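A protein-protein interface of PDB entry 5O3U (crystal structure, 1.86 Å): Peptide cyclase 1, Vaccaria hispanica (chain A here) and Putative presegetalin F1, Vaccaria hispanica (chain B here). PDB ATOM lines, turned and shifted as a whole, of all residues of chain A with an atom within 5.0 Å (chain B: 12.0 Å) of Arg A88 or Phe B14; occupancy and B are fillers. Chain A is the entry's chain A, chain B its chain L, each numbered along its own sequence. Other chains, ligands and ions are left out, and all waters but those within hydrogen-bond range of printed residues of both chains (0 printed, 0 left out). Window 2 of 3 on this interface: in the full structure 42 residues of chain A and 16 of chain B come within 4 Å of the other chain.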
ATOM      1  N   PHE A  86      22.119  24.488  22.230  1.00  0.00           N
ATOM      2  CA  PHE A  86      21.922  25.282  23.411  1.00  0.00           C
ATOM      3  C   PHE A  86      23.127  25.185  24.325  1.00  0.00           C
ATOM      4  O   PHE A  86      23.892  24.215  24.261  1.00  0.00           O
ATOM      5  CB  PHE A  86      20.613  24.930  24.124  1.00  0.00           C
ATOM      6  CG  PHE A  86      20.542  23.543  24.703  1.00  0.00           C
ATOM      7  CD1 PHE A  86      20.926  23.300  26.017  1.00  0.00           C
ATOM      8  CD2 PHE A  86      20.006  22.496  23.957  1.00  0.00           C
ATOM      9  CE1 PHE A  86      20.833  22.027  26.565  1.00  0.00           C
ATOM     10  CE2 PHE A  86      19.910  21.229  24.497  1.00  0.00           C
ATOM     11  CZ  PHE A  86      20.313  20.999  25.811  1.00  0.00           C
ATOM     12  N   ARG A  87      23.285  26.209  25.146  1.00  0.00           N
ATOM     13  CA  ARG A  87      24.470  26.348  25.947  1.00  0.00           C
ATOM     14  C   ARG A  87      24.196  26.097  27.426  1.00  0.00           C
ATOM     15  O   ARG A  87      23.226  26.610  27.969  1.00  0.00           O
ATOM     16  CB  ARG A  87      25.034  27.745  25.749  1.00  0.00           C
ATOM     17  CG  ARG A  87      26.326  27.963  26.495  1.00  0.00           C
ATOM     18  CD  ARG A  87      26.927  29.294  26.098  1.00  0.00           C
ATOM     19  NE  ARG A  87      27.891  29.769  27.063  1.00  0.00           N
ATOM     20  CZ  ARG A  87      28.716  30.789  26.866  1.00  0.00           C
ATOM     21  NH1 ARG A  87      28.749  31.430  25.690  1.00  0.00           N
ATOM     22  NH2 ARG A  87      29.572  31.125  27.841  1.00  0.00           N
ATOM     23  N   ARG A  88      25.062  25.311  28.075  1.00  0.00           N
ATOM     24  CA  ARG A  88      25.116  25.236  29.517  1.00  0.00           C
ATOM     25  C   ARG A  88      26.567  25.339  29.956  1.00  0.00           C
ATOM     26  O   ARG A  88      27.436  24.667  29.405  1.00  0.00           O
ATOM     27  CB  ARG A  88      24.543  23.931  30.053  1.00  0.00           C
ATOM     28  CG  ARG A  88      23.096  23.682  29.726  1.00  0.00           C
ATOM     29  CD  ARG A  88      22.135  24.480  30.601  1.00  0.00           C
ATOM     30  NE  ARG A  88      20.763  24.217  30.174  1.00  0.00           N
ATOM     31  CZ  ARG A  88      20.085  24.875  29.229  1.00  0.00           C
ATOM     32  NH1 ARG A  88      20.597  25.911  28.576  1.00  0.00           N
ATOM     33  NH2 ARG A  88      18.845  24.491  28.961  1.00  0.00           N
ATOM     34  N   ALA A  89      26.834  26.190  30.952  1.00  0.00           N
ATOM     35  CA  ALA A  89      28.188  26.548  31.321  1.00  0.00           C
ATOM     36  C   ALA A  89      28.950  26.955  30.049  1.00  0.00           C
ATOM     37  O   ALA A  89      28.484  27.811  29.338  1.00  0.00           O
ATOM     38  CB  ALA A  89      28.843  25.403  32.134  1.00  0.00           C
ATOM     39  N   ASN A  90      30.058  26.312  29.723  1.00  0.00           N
ATOM     40  CA  ASN A  90      30.763  26.580  28.446  1.00  0.00           C
ATOM     41  C   ASN A  90      30.709  25.401  27.485  1.00  0.00           C
ATOM     42  O   ASN A  90      31.615  25.202  26.680  1.00  0.00           O
ATOM     43  CB  ASN A  90      32.230  26.969  28.723  1.00  0.00           C
ATOM     44  CG  ASN A  90      32.342  28.312  29.391  1.00  0.00           C
ATOM     45  OD1 ASN A  90      31.693  29.262  28.928  1.00  0.00           O
ATOM     46  ND2 ASN A  90      33.100  28.423  30.469  1.00  0.00           N
ATOM     47  N   LYS A  91      29.627  24.654  27.529  1.00  0.00           N
ATOM     48  CA  LYS A  91      29.401  23.508  26.644  1.00  0.00           C
ATOM     49  C   LYS A  91      28.181  23.811  25.794  1.00  0.00           C
ATOM     50  O   LYS A  91      27.306  24.567  26.221  1.00  0.00           O
ATOM     51  CB  LYS A  91      29.141  22.238  27.460  1.00  0.00           C
ATOM     52  CG  LYS A  91      30.291  21.801  28.352  1.00  0.00           C
ATOM     53  CD  LYS A  91      31.517  21.269  27.617  1.00  0.00           C
ATOM     54  CE  LYS A  91      32.672  21.025  28.596  1.00  0.00           C
ATOM     55  NZ  LYS A  91      32.278  20.039  29.625  1.00  0.00           N
ATOM     56  N   PHE A  93      25.186  21.874  23.270  1.00  0.00           N
ATOM     57  CA  PHE A  93      24.493  20.610  23.131  1.00  0.00           C
ATOM     58  C   PHE A  93      23.512  20.699  21.980  1.00  0.00           C
ATOM     59  O   PHE A  93      22.886  21.720  21.781  1.00  0.00           O
ATOM     60  CB  PHE A  93      23.702  20.311  24.413  1.00  0.00           C
ATOM     61  CG  PHE A  93      24.553  20.188  25.637  1.00  0.00           C
ATOM     62  CD1 PHE A  93      24.883  21.300  26.389  1.00  0.00           C
ATOM     63  CD2 PHE A  93      25.058  18.954  26.017  1.00  0.00           C
ATOM     64  CE1 PHE A  93      25.722  21.177  27.489  1.00  0.00           C
ATOM     65  CE2 PHE A  93      25.877  18.830  27.122  1.00  0.00           C
ATOM     66  CZ  PHE A  93      26.210  19.946  27.855  1.00  0.00           C
ATOM     67  N   SER A 133      12.413  12.391  24.238  1.00  0.00           N
ATOM     68  CA  SER A 133      11.445  13.482  24.405  1.00  0.00           C
ATOM     69  C   SER A 133      11.801  14.448  25.546  1.00  0.00           C
ATOM     70  O   SER A 133      11.560  15.647  25.455  1.00  0.00           O
ATOM     71  CB  SER A 133      10.043  12.908  24.597  1.00  0.00           C
ATOM     72  OG  SER A 133       9.965  12.043  25.724  1.00  0.00           O
ATOM     73  N   LEU A 134      12.359  13.899  26.613  1.00  0.00           N
ATOM     74  CA  LEU A 134      12.838  14.703  27.754  1.00  0.00           C
ATOM     75  C   LEU A 134      14.353  14.715  27.716  1.00  0.00           C
ATOM     76  O   LEU A 134      15.005  13.663  27.582  1.00  0.00           O
ATOM     77  CB  LEU A 134      12.295  14.159  29.078  1.00  0.00           C
ATOM     78  CG  LEU A 134      13.000  14.625  30.351  1.00  0.00           C
ATOM     79  CD1 LEU A 134      12.934  16.146  30.524  1.00  0.00           C
ATOM     80  CD2 LEU A 134      12.377  13.953  31.556  1.00  0.00           C
ATOM     81  N   TYR A 135      14.926  15.904  27.738  1.00  0.00           N
ATOM     82  CA  TYR A 135      16.377  16.040  27.736  1.00  0.00           C
ATOM     83  C   TYR A 135      16.634  17.337  28.472  1.00  0.00           C
ATOM     84  O   TYR A 135      15.920  18.329  28.251  1.00  0.00           O
ATOM     85  CB  TYR A 135      17.006  16.036  26.336  1.00  0.00           C
ATOM     86  CG  TYR A 135      16.237  16.790  25.277  1.00  0.00           C
ATOM     87  CD1 TYR A 135      15.137  16.186  24.637  1.00  0.00           C
ATOM     88  CD2 TYR A 135      16.585  18.084  24.901  1.00  0.00           C
ATOM     89  CE1 TYR A 135      14.428  16.838  23.664  1.00  0.00           C
ATOM     90  CE2 TYR A 135      15.869  18.759  23.916  1.00  0.00           C
ATOM     91  CZ  TYR A 135      14.791  18.140  23.321  1.00  0.00           C
ATOM     92  OH  TYR A 135      14.076  18.799  22.347  1.00  0.00           O
ATOM     93  N   SER A 136      17.532  17.291  29.429  1.00  0.00           N
ATOM     94  CA  SER A 136      17.767  18.444  30.288  1.00  0.00           C
ATOM     95  C   SER A 136      19.158  18.356  30.853  1.00  0.00           C
ATOM     96  O   SER A 136      19.521  17.367  31.461  1.00  0.00           O
ATOM     97  CB  SER A 136      16.732  18.439  31.395  1.00  0.00           C
ATOM     98  OG  SER A 136      17.010  19.384  32.369  1.00  0.00           O
ATOM     99  N   VAL A 137      19.911  19.440  30.706  1.00  0.00           N
ATOM    100  CA  VAL A 137      21.304  19.464  31.110  1.00  0.00           C
ATOM    101  C   VAL A 137      21.373  20.418  32.297  1.00  0.00           C
ATOM    102  O   VAL A 137      20.757  21.493  32.270  1.00  0.00           O
ATOM    103  CB  VAL A 137      22.212  19.908  29.950  1.00  0.00           C
ATOM    104  CG1 VAL A 137      23.653  20.082  30.400  1.00  0.00           C
ATOM    105  CG2 VAL A 137      22.139  18.918  28.796  1.00  0.00           C
ATOM    106  N   SER A 138      22.082  20.014  33.325  1.00  0.00           N
ATOM    107  CA  SER A 138      22.299  20.827  34.517  1.00  0.00           C
ATOM    108  C   SER A 138      23.056  22.123  34.202  1.00  0.00           C
ATOM    109  O   SER A 138      23.743  22.248  33.158  1.00  0.00           O
ATOM    110  CB  SER A 138      23.069  20.025  35.576  1.00  0.00           C
ATOM    111  OG  SER A 138      24.392  19.757  35.136  1.00  0.00           O
ATOM    112  N   GLU A 139      22.909  23.098  35.104  1.00  0.00           N
ATOM    113  CA  GLU A 139      23.527  24.426  34.914  1.00  0.00           C
ATOM    114  C   GLU A 139      25.049  24.393  34.762  1.00  0.00           C
ATOM    115  O   GLU A 139      25.602  25.142  33.959  1.00  0.00           O
ATOM    116  CB  GLU A 139      23.138  25.373  36.053  1.00  0.00           C
ATOM    117  CG  GLU A 139      21.688  25.760  36.024  1.00  0.00           C
ATOM    118  CD  GLU A 139      21.310  26.580  34.781  1.00  0.00           C
ATOM    119  OE1 GLU A 139      21.858  27.692  34.563  1.00  0.00           O
ATOM    120  OE2 GLU A 139      20.453  26.081  34.010  1.00  0.00           O
ATOM    121  N   ALA A 141      26.602  21.899  33.498  1.00  0.00           N
ATOM    122  CA  ALA A 141      26.820  21.002  32.375  1.00  0.00           C
ATOM    123  C   ALA A 141      27.430  19.664  32.753  1.00  0.00           C
ATOM    124  O   ALA A 141      27.907  18.941  31.880  1.00  0.00           O
ATOM    125  CB  ALA A 141      27.623  21.680  31.264  1.00  0.00           C
ATOM    126  N   THR A 394      16.038  28.759  21.923  1.00  0.00           N
ATOM    127  CA  THR A 394      16.307  28.261  23.278  1.00  0.00           C
ATOM    128  C   THR A 394      17.253  29.125  24.140  1.00  0.00           C
ATOM    129  O   THR A 394      17.502  28.769  25.296  1.00  0.00           O
ATOM    130  CB  THR A 394      16.814  26.805  23.234  1.00  0.00           C
ATOM    131  OG1 THR A 394      17.942  26.733  22.359  1.00  0.00           O
ATOM    132  CG2 THR A 394      15.704  25.864  22.671  1.00  0.00           C
ATOM    133  N   ARG A 396      19.003  31.722  26.595  1.00  0.00           N
ATOM    134  CA  ARG A 396      18.597  32.197  27.908  1.00  0.00           C
ATOM    135  C   ARG A 396      19.086  33.620  28.117  1.00  0.00           C
ATOM    136  O   ARG A 396      19.878  34.131  27.345  1.00  0.00           O
ATOM    137  CB  ARG A 396      19.134  31.244  28.995  1.00  0.00           C
ATOM    138  CG  ARG A 396      18.455  29.871  28.857  1.00  0.00           C
ATOM    139  CD  ARG A 396      18.666  28.993  30.046  1.00  0.00           C
ATOM    140  NE  ARG A 396      20.085  28.829  30.375  1.00  0.00           N
ATOM    141  CZ  ARG A 396      20.544  28.009  31.324  1.00  0.00           C
ATOM    142  NH1 ARG A 396      19.717  27.184  31.972  1.00  0.00           N
ATOM    143  NH2 ARG A 396      21.858  27.917  31.530  1.00  0.00           N
ATOM    144  N   PHE B  14      14.326  20.439  28.378  1.00  0.00           N
ATOM    145  CA  PHE B  14      13.200  20.599  27.408  1.00  0.00           C
ATOM    146  C   PHE B  14      12.371  19.311  27.343  1.00  0.00           C
ATOM    147  O   PHE B  14      12.927  18.203  27.340  1.00  0.00           O
ATOM    148  CB  PHE B  14      13.719  20.968  26.006  1.00  0.00           C
ATOM    149  CG  PHE B  14      14.702  22.112  25.998  1.00  0.00           C
ATOM    150  CD1 PHE B  14      14.266  23.443  26.094  1.00  0.00           C
ATOM    151  CD2 PHE B  14      16.074  21.862  25.912  1.00  0.00           C
ATOM    152  CE1 PHE B  14      15.185  24.489  26.103  1.00  0.00           C
ATOM    153  CE2 PHE B  14      16.993  22.906  25.903  1.00  0.00           C
ATOM    154  CZ  PHE B  14      16.552  24.220  26.001  1.00  0.00           C
ATOM    155  N   SER B  15      11.049  19.468  27.308  1.00  0.00           N
ATOM    156  CA  SER B  15      10.114  18.340  27.310  1.00  0.00           C
ATOM    157  C   SER B  15       8.986  18.553  26.293  1.00  0.00           C
ATOM    158  O   SER B  15       8.813  19.665  25.772  1.00  0.00           O
ATOM    159  CB  SER B  15       9.550  18.142  28.716  1.00  0.00           C
ATOM    160  OG  SER B  15       8.959  19.339  29.206  1.00  0.00           O
ATOM    161  N   ALA B  16       8.237  17.479  26.021  1.00  0.00           N
ATOM    162  CA  ALA B  16       7.265  17.429  24.906  1.00  0.00           C
ATOM    163  C   ALA B  16       6.146  18.483  24.991  1.00  0.00           C
ATOM    164  O   ALA B  16       5.472  18.599  26.019  1.00  0.00           O
ATOM    165  CB  ALA B  16       6.658  16.032  24.792  1.00  0.00           C
ATOM    166  N   SER B  17       5.964  19.228  23.896  1.00  0.00           N
ATOM    167  CA  SER B  17       4.910  20.254  23.776  1.00  0.00           C
ATOM    168  C   SER B  17       3.573  19.668  23.283  1.00  0.00           C
ATOM    169  O   SER B  17       3.534  18.559  22.735  1.00  0.00           O
ATOM    170  CB  SER B  17       5.352  21.389  22.829  1.00  0.00           C
ATOM    171  OG  SER B  17       6.243  22.285  23.477  1.00  0.00           O
ATOM    172  N   TYR B  18       2.496  20.436  23.494  1.00  0.00           N
ATOM    173  CA  TYR B  18       1.125  20.108  23.035  1.00  0.00           C
ATOM    174  C   TYR B  18       0.570  18.801  23.615  1.00  0.00           C
ATOM    175  O   TYR B  18      -0.338  18.202  23.041  1.00  0.00           O
ATOM    176  CB  TYR B  18       1.054  20.042  21.489  1.00  0.00           C
ATOM    177  CG  TYR B  18       1.718  21.204  20.781  1.00  0.00           C
ATOM    178  CD1 TYR B  18       1.410  22.530  21.124  1.00  0.00           C
ATOM    179  CD2 TYR B  18       2.649  20.983  19.756  1.00  0.00           C
ATOM    180  CE1 TYR B  18       2.023  23.596  20.479  1.00  0.00           C
ATOM    181  CE2 TYR B  18       3.259  22.043  19.100  1.00  0.00           C
ATOM    182  CZ  TYR B  18       2.944  23.348  19.465  1.00  0.00           C
ATOM    183  OH  TYR B  18       3.544  24.405  18.822  1.00  0.00           O
ATOM    184  N   SER B  19       1.094  18.382  24.764  1.00  0.00           N
ATOM    185  CA  SER B  19       0.954  17.004  25.225  1.00  0.00           C
ATOM    186  C   SER B  19      -0.471  16.553  25.546  1.00  0.00           C
ATOM    187  O   SER B  19      -0.779  15.364  25.480  1.00  0.00           O
ATOM    188  CB  SER B  19       1.841  16.778  26.458  1.00  0.00           C
ATOM    189  OG  SER B  19       1.359  17.483  27.595  1.00  0.00           O
ATOM    190  N   ASN B  33      11.483  16.618  18.324  1.00  0.00           N
ATOM    191  CA  ASN B  33      12.682  15.809  18.095  1.00  0.00           C
ATOM    192  C   ASN B  33      12.412  14.602  17.163  1.00  0.00           C
ATOM    193  O   ASN B  33      12.911  13.469  17.387  1.00  0.00           O
ATOM    194  CB  ASN B  33      13.262  15.353  19.443  1.00  0.00           C
ATOM    195  CG  ASN B  33      14.667  14.773  19.323  1.00  0.00           C
ATOM    196  OD1 ASN B  33      15.442  15.199  18.477  1.00  0.00           O
ATOM    197  ND2 ASN B  33      14.989  13.786  20.157  1.00  0.00           N
ATOM    198  N   ALA B  34      11.643  14.863  16.105  1.00  0.00           N
ATOM    199  CA  ALA B  34      11.389  13.860  15.089  1.00  0.00           C
ATOM    200  C   ALA B  34      12.713  13.472  14.424  1.00  0.00           C
ATOM    201  O   ALA B  34      13.583  14.318  14.204  1.00  0.00           O
ATOM    202  CB  ALA B  34      10.386  14.364  14.038  1.00  0.00           C
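N of Phe B14 is in hydrogen-bond range of O of Tyr A135 (2.6 Å). O of Phe B14 lies close to O of Ser A133 (3.5 Å).
Of chain B, only Phe B14 comes within 4 Å of Arg A88. No residue of chain B comes within 4 Å of Arg A87. No residue of chain B comes within 4 Å of Asn A90. No residue of chain B comes within 4 Å of Phe A93. Ser A133 touches just these residues of chain B: Phe B14 (3.5 Å), Ser B15 (3.6 Å) and Ala B16 (3.8 Å). Of the printed residues of chain B, Leu A134 touches Phe B14. No residue of chain B comes within 4 Å of Ser A136. No residue of chain B comes within 4 Å of Val A137. No residue of chain B comes within 4 Å of Ser A138. No residue of chain B comes within 4 Å of Ala A141. Thr A394 touches just one residue of chain B: Phe B14 (3.7 Å). Of the printed residues of chain A, Ser B15 touches Ser A133 (3.6 Å). Of the printed residues of chain A, Ala B16 touches Ser A133. Asn B33 touches none of the printed residues of chain A. The nearest residue of chain A that does not touch Phe B14 is Ser A136 (4.3 Å).
Hydrophobic or aromatic side chains of chain B within 4 Å of the printed part of chain A: Phe B14. Hydrophobic or aromatic side chains of chain A that line the printed part of chain B: Phe A86, Leu A134 and Tyr A135. Among the printed residues, 8 pairs touch across the chains. Among the printed residues, no Asp or Glu carboxylate lies within 4 Å of a Lys or Arg side-chain nitrogen of the other chain.
The guanidinium group of Arg A88 is in hydrogen-bond range of the backbone carbonyl oxygen of Val A137 (3.4 Å). The backbone carbonyl oxygen (O) of Phe A86 lies within hydrogen-bond range of the backbone NH (N) of Phe A93.
Among the printed residues, pairs that only touch across the chains: Phe A86 with Phe B14, Arg A88 with Phe B14, Ser A133 with Ser B15, Ser A133 with Ala B16, Leu A134 with Phe B14 and Thr A394 with Phe B14.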
